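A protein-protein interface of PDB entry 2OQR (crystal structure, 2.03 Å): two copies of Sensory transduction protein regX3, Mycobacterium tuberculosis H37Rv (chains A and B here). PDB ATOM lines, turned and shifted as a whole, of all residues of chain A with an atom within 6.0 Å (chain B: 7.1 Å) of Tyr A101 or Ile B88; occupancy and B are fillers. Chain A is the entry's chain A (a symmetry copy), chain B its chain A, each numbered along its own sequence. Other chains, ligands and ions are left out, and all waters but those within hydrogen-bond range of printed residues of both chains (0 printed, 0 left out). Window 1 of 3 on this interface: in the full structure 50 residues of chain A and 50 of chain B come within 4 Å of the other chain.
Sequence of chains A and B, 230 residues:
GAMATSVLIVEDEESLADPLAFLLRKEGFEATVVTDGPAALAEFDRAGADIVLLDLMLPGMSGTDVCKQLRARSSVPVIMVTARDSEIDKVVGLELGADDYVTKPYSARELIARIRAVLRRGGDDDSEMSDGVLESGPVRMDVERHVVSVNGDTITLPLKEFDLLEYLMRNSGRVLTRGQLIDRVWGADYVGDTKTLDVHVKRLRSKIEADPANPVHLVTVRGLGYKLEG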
ATOM      1  N   ASP A  85      28.423 -29.491  18.438  1.00  0.00           N
ATOM      2  CA  ASP A  85      27.178 -29.512  19.212  1.00  0.00           C
ATOM      3  C   ASP A  85      27.382 -28.736  20.499  1.00  0.00           C
ATOM      4  O   ASP A  85      26.585 -27.903  20.853  1.00  0.00           O
ATOM      5  CB  ASP A  85      26.804 -30.964  19.552  1.00  0.00           C
ATOM      6  CG  ASP A  85      26.494 -31.799  18.316  1.00  0.00           C
ATOM      7  OD1 ASP A  85      25.985 -31.242  17.305  1.00  0.00           O
ATOM      8  OD2 ASP A  85      26.726 -33.036  18.373  1.00  0.00           O
ATOM      9  N   ILE A  88      27.699 -24.727  19.949  1.00  0.00           N
ATOM     10  CA  ILE A  88      26.426 -24.028  19.719  1.00  0.00           C
ATOM     11  C   ILE A  88      25.571 -24.049  20.994  1.00  0.00           C
ATOM     12  O   ILE A  88      24.854 -23.091  21.280  1.00  0.00           O
ATOM     13  CB  ILE A  88      25.659 -24.581  18.490  1.00  0.00           C
ATOM     14  CG1 ILE A  88      24.444 -23.720  18.183  1.00  0.00           C
ATOM     15  CG2 ILE A  88      25.254 -26.022  18.707  1.00  0.00           C
ATOM     16  CD1 ILE A  88      24.750 -22.311  17.910  1.00  0.00           C
ATOM     17  N   ASP A  89      25.691 -25.108  21.786  1.00  0.00           N
ATOM     18  CA  ASP A  89      24.972 -25.172  23.081  1.00  0.00           C
ATOM     19  C   ASP A  89      25.499 -24.021  23.991  1.00  0.00           C
ATOM     20  O   ASP A  89      24.724 -23.265  24.618  1.00  0.00           O
ATOM     21  CB  ASP A  89      25.105 -26.576  23.742  1.00  0.00           C
ATOM     22  CG  ASP A  89      24.228 -27.678  23.093  1.00  0.00           C
ATOM     23  OD1 ASP A  89      23.166 -27.465  22.441  1.00  0.00           O
ATOM     24  OD2 ASP A  89      24.565 -28.864  23.285  1.00  0.00           O
ATOM     25  N   VAL A  92      24.310 -20.406  22.535  1.00  0.00           N
ATOM     26  CA  VAL A  92      22.917 -20.014  22.768  1.00  0.00           C
ATOM     27  C   VAL A  92      22.687 -19.709  24.242  1.00  0.00           C
ATOM     28  O   VAL A  92      21.772 -18.956  24.605  1.00  0.00           O
ATOM     29  CB  VAL A  92      21.913 -21.072  22.248  1.00  0.00           C
ATOM     30  CG1 VAL A  92      22.119 -21.258  20.757  1.00  0.00           C
ATOM     31  CG2 VAL A  92      22.027 -22.382  23.018  1.00  0.00           C
ATOM     32  N   ALA A  98      19.480 -19.639  26.568  1.00  0.00           N
ATOM     33  CA  ALA A  98      18.920 -20.961  26.304  1.00  0.00           C
ATOM     34  C   ALA A  98      19.741 -22.061  26.980  1.00  0.00           C
ATOM     35  O   ALA A  98      20.968 -21.933  27.159  1.00  0.00           O
ATOM     36  CB  ALA A  98      18.859 -21.200  24.805  1.00  0.00           C
ATOM     37  N   ASP A  99      19.090 -23.164  27.332  1.00  0.00           N
ATOM     38  CA  ASP A  99      19.798 -24.245  28.009  1.00  0.00           C
ATOM     39  C   ASP A  99      20.401 -25.229  27.010  1.00  0.00           C
ATOM     40  O   ASP A  99      21.285 -25.997  27.348  1.00  0.00           O
ATOM     41  CB  ASP A  99      18.866 -24.997  28.957  1.00  0.00           C
ATOM     42  CG  ASP A  99      18.516 -24.192  30.179  1.00  0.00           C
ATOM     43  OD1 ASP A  99      19.275 -24.300  31.158  1.00  0.00           O
ATOM     44  OD2 ASP A  99      17.510 -23.441  30.148  1.00  0.00           O
ATOM     45  N   ASP A 100      19.889 -25.240  25.794  1.00  0.00           N
ATOM     46  CA  ASP A 100      20.341 -26.223  24.839  1.00  0.00           C
ATOM     47  C   ASP A 100      19.874 -25.796  23.482  1.00  0.00           C
ATOM     48  O   ASP A 100      18.898 -25.060  23.338  1.00  0.00           O
ATOM     49  CB  ASP A 100      19.794 -27.625  25.207  1.00  0.00           C
ATOM     50  CG  ASP A 100      20.354 -28.753  24.325  1.00  0.00           C
ATOM     51  OD1 ASP A 100      19.582 -29.652  23.951  1.00  0.00           O
ATOM     52  OD2 ASP A 100      21.554 -28.778  24.042  1.00  0.00           O
ATOM     53  N   TYR A 101      20.638 -26.222  22.494  1.00  0.00           N
ATOM     54  CA  TYR A 101      20.291 -26.124  21.114  1.00  0.00           C
ATOM     55  C   TYR A 101      20.089 -27.532  20.573  1.00  0.00           C
ATOM     56  O   TYR A 101      20.909 -28.436  20.821  1.00  0.00           O
ATOM     57  CB  TYR A 101      21.452 -25.479  20.360  1.00  0.00           C
ATOM     58  CG  TYR A 101      21.270 -25.456  18.871  1.00  0.00           C
ATOM     59  CD1 TYR A 101      21.717 -26.508  18.082  1.00  0.00           C
ATOM     60  CD2 TYR A 101      20.665 -24.392  18.239  1.00  0.00           C
ATOM     61  CE1 TYR A 101      21.537 -26.491  16.700  1.00  0.00           C
ATOM     62  CE2 TYR A 101      20.500 -24.375  16.858  1.00  0.00           C
ATOM     63  CZ  TYR A 101      20.943 -25.437  16.100  1.00  0.00           C
ATOM     64  OH  TYR A 101      20.829 -25.467  14.704  1.00  0.00           O
ATOM     65  N   VAL A 102      19.026 -27.729  19.808  1.00  0.00           N
ATOM     66  CA  VAL A 102      18.797 -29.006  19.173  1.00  0.00           C
ATOM     67  C   VAL A 102      18.416 -28.846  17.687  1.00  0.00           C
ATOM     68  O   VAL A 102      17.690 -27.935  17.327  1.00  0.00           O
ATOM     69  CB  VAL A 102      17.877 -29.935  20.010  1.00  0.00           C
ATOM     70  CG1 VAL A 102      17.329 -29.251  21.291  1.00  0.00           C
ATOM     71  CG2 VAL A 102      16.844 -30.578  19.206  1.00  0.00           C
ATOM     72  N   THR A 103      19.050 -29.668  16.837  1.00  0.00           N
ATOM     73  CA  THR A 103      18.776 -29.687  15.412  1.00  0.00           C
ATOM     74  C   THR A 103      17.511 -30.463  15.206  1.00  0.00           C
ATOM     75  O   THR A 103      17.333 -31.504  15.796  1.00  0.00           O
ATOM     76  CB  THR A 103      19.927 -30.295  14.599  1.00  0.00           C
ATOM     77  OG1 THR A 103      21.140 -29.632  14.970  1.00  0.00           O
ATOM     78  CG2 THR A 103      19.689 -30.061  13.067  1.00  0.00           C
ATOM     79  N   ARG A 114      15.227 -36.579  27.605  1.00  0.00           N
ATOM     80  CA  ARG A 114      16.096 -35.501  28.093  1.00  0.00           C
ATOM     81  C   ARG A 114      15.384 -34.559  29.077  1.00  0.00           C
ATOM     82  O   ARG A 114      15.953 -34.091  30.047  1.00  0.00           O
ATOM     83  CB  ARG A 114      16.623 -34.712  26.922  1.00  0.00           C
ATOM     84  CG  ARG A 114      17.474 -35.583  26.021  1.00  0.00           C
ATOM     85  CD  ARG A 114      18.026 -34.790  24.923  1.00  0.00           C
ATOM     86  NE  ARG A 114      18.877 -33.748  25.463  1.00  0.00           N
ATOM     87  CZ  ARG A 114      19.476 -32.827  24.731  1.00  0.00           C
ATOM     88  NH1 ARG A 114      19.313 -32.806  23.412  1.00  0.00           N
ATOM     89  NH2 ARG A 114      20.222 -31.919  25.332  1.00  0.00           N
ATOM     90  N   LEU B  56      13.616 -21.698  16.610  1.00  0.00           N
ATOM     91  CA  LEU B  56      14.556 -20.569  16.479  1.00  0.00           C
ATOM     92  C   LEU B  56      14.146 -19.598  15.372  1.00  0.00           C
ATOM     93  O   LEU B  56      14.509 -18.404  15.412  1.00  0.00           O
ATOM     94  CB  LEU B  56      15.933 -21.116  16.162  1.00  0.00           C
ATOM     95  CG  LEU B  56      17.221 -20.532  16.731  1.00  0.00           C
ATOM     96  CD1 LEU B  56      18.329 -20.805  15.706  1.00  0.00           C
ATOM     97  CD2 LEU B  56      17.123 -19.076  17.106  1.00  0.00           C
ATOM     98  N   MET B  57      13.441 -20.116  14.362  1.00  0.00           N
ATOM     99  CA  MET B  57      12.947 -19.289  13.257  1.00  0.00           C
ATOM    100  C   MET B  57      11.418 -19.284  13.228  1.00  0.00           C
ATOM    101  O   MET B  57      10.737 -20.344  13.017  1.00  0.00           O
ATOM    102  CB  MET B  57      13.525 -19.795  11.930  1.00  0.00           C
ATOM    103  CG  MET B  57      13.270 -18.936  10.713  1.00  0.00           C
ATOM    104  SD  MET B  57      14.702 -17.937  10.265  1.00  0.00           S
ATOM    105  CE  MET B  57      14.811 -16.834  11.668  1.00  0.00           C
ATOM    106  N   ILE B  79      14.936 -23.720  28.680  1.00  0.00           N
ATOM    107  CA  ILE B  79      14.586 -23.250  27.356  1.00  0.00           C
ATOM    108  C   ILE B  79      15.515 -23.952  26.366  1.00  0.00           C
ATOM    109  O   ILE B  79      16.722 -23.772  26.424  1.00  0.00           O
ATOM    110  CB  ILE B  79      14.755 -21.748  27.210  1.00  0.00           C
ATOM    111  CG1 ILE B  79      13.847 -20.967  28.168  1.00  0.00           C
ATOM    112  CG2 ILE B  79      14.398 -21.329  25.812  1.00  0.00           C
ATOM    113  CD1 ILE B  79      14.140 -19.496  28.197  1.00  0.00           C
ATOM    114  N   MET B  80      14.936 -24.769  25.492  1.00  0.00           N
ATOM    115  CA  MET B  80      15.669 -25.461  24.434  1.00  0.00           C
ATOM    116  C   MET B  80      15.242 -24.895  23.090  1.00  0.00           C
ATOM    117  O   MET B  80      14.044 -24.904  22.762  1.00  0.00           O
ATOM    118  CB  MET B  80      15.400 -26.964  24.499  1.00  0.00           C
ATOM    119  CG  MET B  80      15.714 -27.590  25.893  1.00  0.00           C
ATOM    120  SD  MET B  80      15.259 -29.354  25.966  1.00  0.00           S
ATOM    121  CE  MET B  80      16.748 -30.020  25.208  1.00  0.00           C
ATOM    122  N   VAL B  81      16.204 -24.339  22.361  1.00  0.00           N
ATOM    123  CA  VAL B  81      15.990 -23.780  21.022  1.00  0.00           C
ATOM    124  C   VAL B  81      16.236 -24.851  19.933  1.00  0.00           C
ATOM    125  O   VAL B  81      17.178 -25.652  20.008  1.00  0.00           O
ATOM    126  CB  VAL B  81      16.851 -22.507  20.771  1.00  0.00           C
ATOM    127  CG1 VAL B  81      16.435 -21.389  21.690  1.00  0.00           C
ATOM    128  CG2 VAL B  81      18.297 -22.775  20.988  1.00  0.00           C
ATOM    129  N   THR B  82      15.367 -24.881  18.931  1.00  0.00           N
ATOM    130  CA  THR B  82      15.368 -25.941  17.941  1.00  0.00           C
ATOM    131  C   THR B  82      15.456 -25.317  16.556  1.00  0.00           C
ATOM    132  O   THR B  82      14.832 -24.295  16.292  1.00  0.00           O
ATOM    133  CB  THR B  82      14.094 -26.834  18.031  1.00  0.00           C
ATOM    134  OG1 THR B  82      12.940 -26.097  17.623  1.00  0.00           O
ATOM    135  CG2 THR B  82      13.842 -27.354  19.447  1.00  0.00           C
ATOM    136  N   ALA B  83      16.218 -25.927  15.656  1.00  0.00           N
ATOM    137  CA  ALA B  83      16.321 -25.368  14.318  1.00  0.00           C
ATOM    138  C   ALA B  83      16.653 -26.446  13.326  1.00  0.00           C
ATOM    139  O   ALA B  83      17.509 -27.271  13.594  1.00  0.00           O
ATOM    140  CB  ALA B  83      17.397 -24.237  14.297  1.00  0.00           C
ATOM    141  N   ARG B  84      15.981 -26.431  12.181  1.00  0.00           N
ATOM    142  CA  ARG B  84      16.457 -27.185  11.002  1.00  0.00           C
ATOM    143  C   ARG B  84      17.790 -26.639  10.513  1.00  0.00           C
ATOM    144  O   ARG B  84      18.121 -25.494  10.760  1.00  0.00           O
ATOM    145  CB  ARG B  84      15.444 -27.100   9.873  1.00  0.00           C
ATOM    146  CG  ARG B  84      14.046 -27.616  10.199  1.00  0.00           C
ATOM    147  CD  ARG B  84      13.095 -27.430   9.036  1.00  0.00           C
ATOM    148  NE  ARG B  84      11.845 -28.162   9.257  1.00  0.00           N
ATOM    149  CZ  ARG B  84      11.656 -29.464   9.010  1.00  0.00           C
ATOM    150  NH1 ARG B  84      12.603 -30.208   8.487  1.00  0.00           N
ATOM    151  NH2 ARG B  84      10.471 -30.025   9.248  1.00  0.00           N
ATOM    152  N   ASP B  85      18.541 -27.448   9.778  1.00  0.00           N
ATOM    153  CA  ASP B  85      19.769 -26.976   9.129  1.00  0.00           C
ATOM    154  C   ASP B  85      19.485 -25.662   8.427  1.00  0.00           C
ATOM    155  O   ASP B  85      20.214 -24.713   8.571  1.00  0.00           O
ATOM    156  CB  ASP B  85      20.238 -28.011   8.094  1.00  0.00           C
ATOM    157  CG  ASP B  85      20.630 -29.342   8.725  1.00  0.00           C
ATOM    158  OD1 ASP B  85      21.119 -29.354   9.888  1.00  0.00           O
ATOM    159  OD2 ASP B  85      20.485 -30.383   8.031  1.00  0.00           O
ATOM    160  N   SER B  86      18.371 -25.608   7.701  1.00  0.00           N
ATOM    161  CA  SER B  86      18.035 -24.428   6.909  1.00  0.00           C
ATOM    162  C   SER B  86      17.663 -23.215   7.746  1.00  0.00           C
ATOM    163  O   SER B  86      17.866 -22.077   7.317  1.00  0.00           O
ATOM    164  CB  SER B  86      16.898 -24.767   5.958  1.00  0.00           C
ATOM    165  OG  SER B  86      15.772 -25.215   6.686  1.00  0.00           O
ATOM    166  N   GLU B  87      17.120 -23.439   8.943  1.00  0.00           N
ATOM    167  CA  GLU B  87      16.767 -22.318   9.815  1.00  0.00           C
ATOM    168  C   GLU B  87      17.992 -21.721  10.499  1.00  0.00           C
ATOM    169  O   GLU B  87      18.117 -20.497  10.627  1.00  0.00           O
ATOM    170  CB  GLU B  87      15.770 -22.764  10.869  1.00  0.00           C
ATOM    171  CG  GLU B  87      14.417 -23.107  10.293  1.00  0.00           C
ATOM    172  CD  GLU B  87      13.467 -23.606  11.365  1.00  0.00           C
ATOM    173  OE1 GLU B  87      13.832 -24.570  12.072  1.00  0.00           O
ATOM    174  OE2 GLU B  87      12.345 -23.048  11.469  1.00  0.00           O
ATOM    175  N   ILE B  88      18.896 -22.552  10.967  1.00  0.00           N
ATOM    176  CA  ILE B  88      20.121 -21.985  11.551  1.00  0.00           C
ATOM    177  C   ILE B  88      20.950 -21.282  10.466  1.00  0.00           C
ATOM    178  O   ILE B  88      21.591 -20.266  10.732  1.00  0.00           O
ATOM    179  CB  ILE B  88      20.949 -23.039  12.331  1.00  0.00           C
ATOM    180  CG1 ILE B  88      22.106 -22.378  13.064  1.00  0.00           C
ATOM    181  CG2 ILE B  88      21.450 -24.126  11.407  1.00  0.00           C
ATOM    182  CD1 ILE B  88      21.707 -21.340  14.021  1.00  0.00           C
ATOM    183  N   ASP B  89      20.890 -21.784   9.239  1.00  0.00           N
ATOM    184  CA  ASP B  89      21.585 -21.117   8.112  1.00  0.00           C
ATOM    185  C   ASP B  89      20.960 -19.701   7.919  1.00  0.00           C
ATOM    186  O   ASP B  89      21.668 -18.677   7.790  1.00  0.00           O
ATOM    187  CB  ASP B  89      21.539 -21.980   6.817  1.00  0.00           C
ATOM    188  CG  ASP B  89      22.504 -23.194   6.819  1.00  0.00           C
ATOM    189  OD1 ASP B  89      23.561 -23.275   7.508  1.00  0.00           O
ATOM    190  OD2 ASP B  89      22.248 -24.129   6.033  1.00  0.00           O
ATOM    191  N   LYS B  90      19.636 -19.616   7.957  1.00  0.00           N
ATOM    192  CA  LYS B  90      18.959 -18.325   7.855  1.00  0.00           C
ATOM    193  C   LYS B  90      19.253 -17.411   9.039  1.00  0.00           C
ATOM    194  O   LYS B  90      19.483 -16.231   8.879  1.00  0.00           O
ATOM    195  CB  LYS B  90      17.441 -18.493   7.758  1.00  0.00           C
ATOM    196  CG  LYS B  90      16.927 -18.889   6.407  1.00  0.00           C
ATOM    197  CD  LYS B  90      15.421 -18.603   6.279  1.00  0.00           C
ATOM    198  CE  LYS B  90      14.627 -19.880   5.956  1.00  0.00           C
ATOM    199  NZ  LYS B  90      14.372 -20.697   7.212  1.00  0.00           N
ATOM    200  N   VAL B  91      19.270 -17.965  10.236  1.00  0.00           N
ATOM    201  CA  VAL B  91      19.486 -17.153  11.404  1.00  0.00           C
ATOM    202  C   VAL B  91      20.884 -16.525  11.391  1.00  0.00           C
ATOM    203  O   VAL B  91      21.030 -15.345  11.673  1.00  0.00           O
ATOM    204  CB  VAL B  91      19.232 -17.963  12.688  1.00  0.00           C
ATOM    205  CG1 VAL B  91      19.652 -17.169  13.930  1.00  0.00           C
ATOM    206  CG2 VAL B  91      17.762 -18.378  12.747  1.00  0.00           C
ATOM    207  N   VAL B  92      21.919 -17.290  11.060  1.00  0.00           N
ATOM    208  CA  VAL B  92      23.276 -16.736  11.092  1.00  0.00           C
ATOM    209  C   VAL B  92      23.455 -15.696   9.994  1.00  0.00           C
ATOM    210  O   VAL B  92      24.307 -14.801  10.091  1.00  0.00           O
ATOM    211  CB  VAL B  92      24.362 -17.836  11.008  1.00  0.00           C
ATOM    212  CG1 VAL B  92      24.200 -18.782  12.183  1.00  0.00           C
ATOM    213  CG2 VAL B  92      24.326 -18.563   9.669  1.00  0.00           C
ATOM    214  N   GLY B  93      22.644 -15.799   8.945  1.00  0.00           N
ATOM    215  CA  GLY B  93      22.631 -14.786   7.905  1.00  0.00           C
ATOM    216  C   GLY B  93      22.062 -13.478   8.442  1.00  0.00           C
ATOM    217  O   GLY B  93      22.683 -12.416   8.347  1.00  0.00           O
ATOM    218  N   LEU B  94      20.872 -13.567   9.019  1.00  0.00           N
ATOM    219  CA  LEU B  94      20.182 -12.384   9.536  1.00  0.00           C
ATOM    220  C   LEU B  94      20.909 -11.803  10.738  1.00  0.00           C
ATOM    221  O   LEU B  94      21.009 -10.602  10.865  1.00  0.00           O
ATOM    222  CB  LEU B  94      18.748 -12.746   9.923  1.00  0.00           C
ATOM    223  CG  LEU B  94      17.778 -13.138   8.799  1.00  0.00           C
ATOM    224  CD1 LEU B  94      16.478 -13.706   9.384  1.00  0.00           C
ATOM    225  CD2 LEU B  94      17.501 -11.940   7.885  1.00  0.00           C
ATOM    226  N   ASP B 100      26.606 -19.410   5.857  1.00  0.00           N
ATOM    227  CA  ASP B 100      26.243 -20.775   6.156  1.00  0.00           C
ATOM    228  C   ASP B 100      26.706 -21.080   7.547  1.00  0.00           C
ATOM    229  O   ASP B 100      27.630 -20.458   8.070  1.00  0.00           O
ATOM    230  CB  ASP B 100      26.881 -21.740   5.126  1.00  0.00           C
ATOM    231  CG  ASP B 100      26.419 -23.198   5.285  1.00  0.00           C
ATOM    232  OD1 ASP B 100      27.260 -24.103   5.154  1.00  0.00           O
ATOM    233  OD2 ASP B 100      25.230 -23.451   5.490  1.00  0.00           O
ATOM    234  N   TYR B 101      25.993 -22.009   8.156  1.00  0.00           N
ATOM    235  CA  TYR B 101      26.360 -22.616   9.393  1.00  0.00           C
ATOM    236  C   TYR B 101      26.671 -24.082   9.131  1.00  0.00           C
ATOM    237  O   TYR B 101      25.913 -24.783   8.435  1.00  0.00           O
ATOM    238  CB  TYR B 101      25.171 -22.539  10.350  1.00  0.00           C
ATOM    239  CG  TYR B 101      25.381 -23.277  11.638  1.00  0.00           C
ATOM    240  CD1 TYR B 101      25.025 -24.614  11.760  1.00  0.00           C
ATOM    241  CD2 TYR B 101      25.921 -22.654  12.742  1.00  0.00           C
ATOM    242  CE1 TYR B 101      25.231 -25.303  12.954  1.00  0.00           C
ATOM    243  CE2 TYR B 101      26.112 -23.344  13.935  1.00  0.00           C
ATOM    244  CZ  TYR B 101      25.760 -24.673  14.024  1.00  0.00           C
ATOM    245  OH  TYR B 101      25.904 -25.413  15.205  1.00  0.00           O
ATOM    246  N   VAL B 102      27.761 -24.570   9.704  1.00  0.00           N
ATOM    247  CA  VAL B 102      28.093 -25.972   9.590  1.00  0.00           C
ATOM    248  C   VAL B 102      28.490 -26.578  10.952  1.00  0.00           C
ATOM    249  O   VAL B 102      29.156 -25.936  11.746  1.00  0.00           O
ATOM    250  CB  VAL B 102      29.059 -26.265   8.412  1.00  0.00           C
ATOM    251  CG1 VAL B 102      29.532 -24.980   7.682  1.00  0.00           C
ATOM    252  CG2 VAL B 102      30.150 -27.157   8.787  1.00  0.00           C
ATOM    253  N   THR B 103      27.933 -27.764  11.240  1.00  0.00           N
ATOM    254  CA  THR B 103      28.236 -28.499  12.455  1.00  0.00           C
ATOM    255  C   THR B 103      29.557 -29.177  12.254  1.00  0.00           C
ATOM    256  O   THR B 103      29.796 -29.747  11.214  1.00  0.00           O
ATOM    257  CB  THR B 103      27.147 -29.520  12.812  1.00  0.00           C
ATOM    258  OG1 THR B 103      25.883 -28.849  12.815  1.00  0.00           O
ATOM    259  CG2 THR B 103      27.398 -30.097  14.248  1.00  0.00           C
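The backbone NH of Leu B56 is in hydrogen-bond range of the backbone carbonyl oxygen of Thr B82.
The backbone NH of Ala A98 sits at hydrogen-bond distance from the backbone carbonyl oxygen of Val A92 (3.1 Å).
OD1 of Asp A100 lies within salt-bridge range of NH2 of Arg A114 (2.7 Å).
Asp A85 touches Thr B103, and with the chains exchanged Thr A103 touches Asp B85.
Ile A88 touches Tyr B101, and with the chains exchanged Tyr A101 touches Ile B88.
Of the 17 pairs that touch across the chains among the printed residues, 4 have their exchanged pair printed and touching as well.
The backbone carbonyl oxygen (O) of Ile B79 sits at hydrogen-bond distance from the backbone NH (N) of Asp A99 (2.6 Å).
O of Asp A100 lies within hydrogen-bond range of N of Val B81 (3.0 Å).
The backbone carbonyl oxygen (O) of Val B81 is in hydrogen-bond range of the backbone NH (N) of Val A102 (2.8 Å).
N of Ala B83 is in hydrogen-bond range of O of Val A102, at 3.0 Å.
Printed residues of chain A that touch a printed residue of chain B: Asp A85, Ile A88, Ala A98, Asp A99, Asp A100, Tyr A101, Val A102, Thr A103 and Arg A114.
Hydrophobic or aromatic side chains of chain A within 4 Å of the printed part of chain B: Ile A88, Ala A98, Tyr A101 and Val A102.
Among the printed residues, 17 pairs touch across the chains.
Among the printed residues, no Asp or Glu carboxylate lies within 4 Å of a Lys or Arg side-chain nitrogen of the other chain.
Of the printed residues of chain B, Ala A98 touches Ile B79 and Val B81.
Of the printed residues of chain B, Tyr A101 touches Val B81 (3.3 Å), Ala B83 (3.7 Å) and Ile B88 (3.4 Å).
Printed residues of chain A within 4 Å of Met B80: Asp A100 and Arg A114.
Of the printed residues of chain A, Val B81 touches Ala A98, Asp A100, Tyr A101 and Val A102.
Of the printed residues of chain A, Asp B85 touches Thr A103 (3.6 Å).
Ile B88 touches just one residue of chain A: Tyr A101.
Printed residues of chain A within 4 Å of Thr B103: Asp A85 (3.6 Å).
Ile A88 touches Tyr B101 (CB to OH, 3.4 Å).
C of Ala A98 touches O of Ile B79, at 3.5 Å.
Ala A98 touches Val B81.
O of Ile B79 touches N of Asp A100, at 3.5 Å.
Tyr A101 touches Val B81.
OH of Tyr A101 touches CB of Ala B83, 3.7 Å away.
OH of Tyr A101 touches CB of Ile B88 (3.4 Å).
Thr B82 touches Val A102 (CA to O, 3.1 Å).
CA of Thr A103 touches O of Ala B83, 3.3 Å away.
Arg A114 touches Met B80 (CZ to CE, 3.9 Å).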
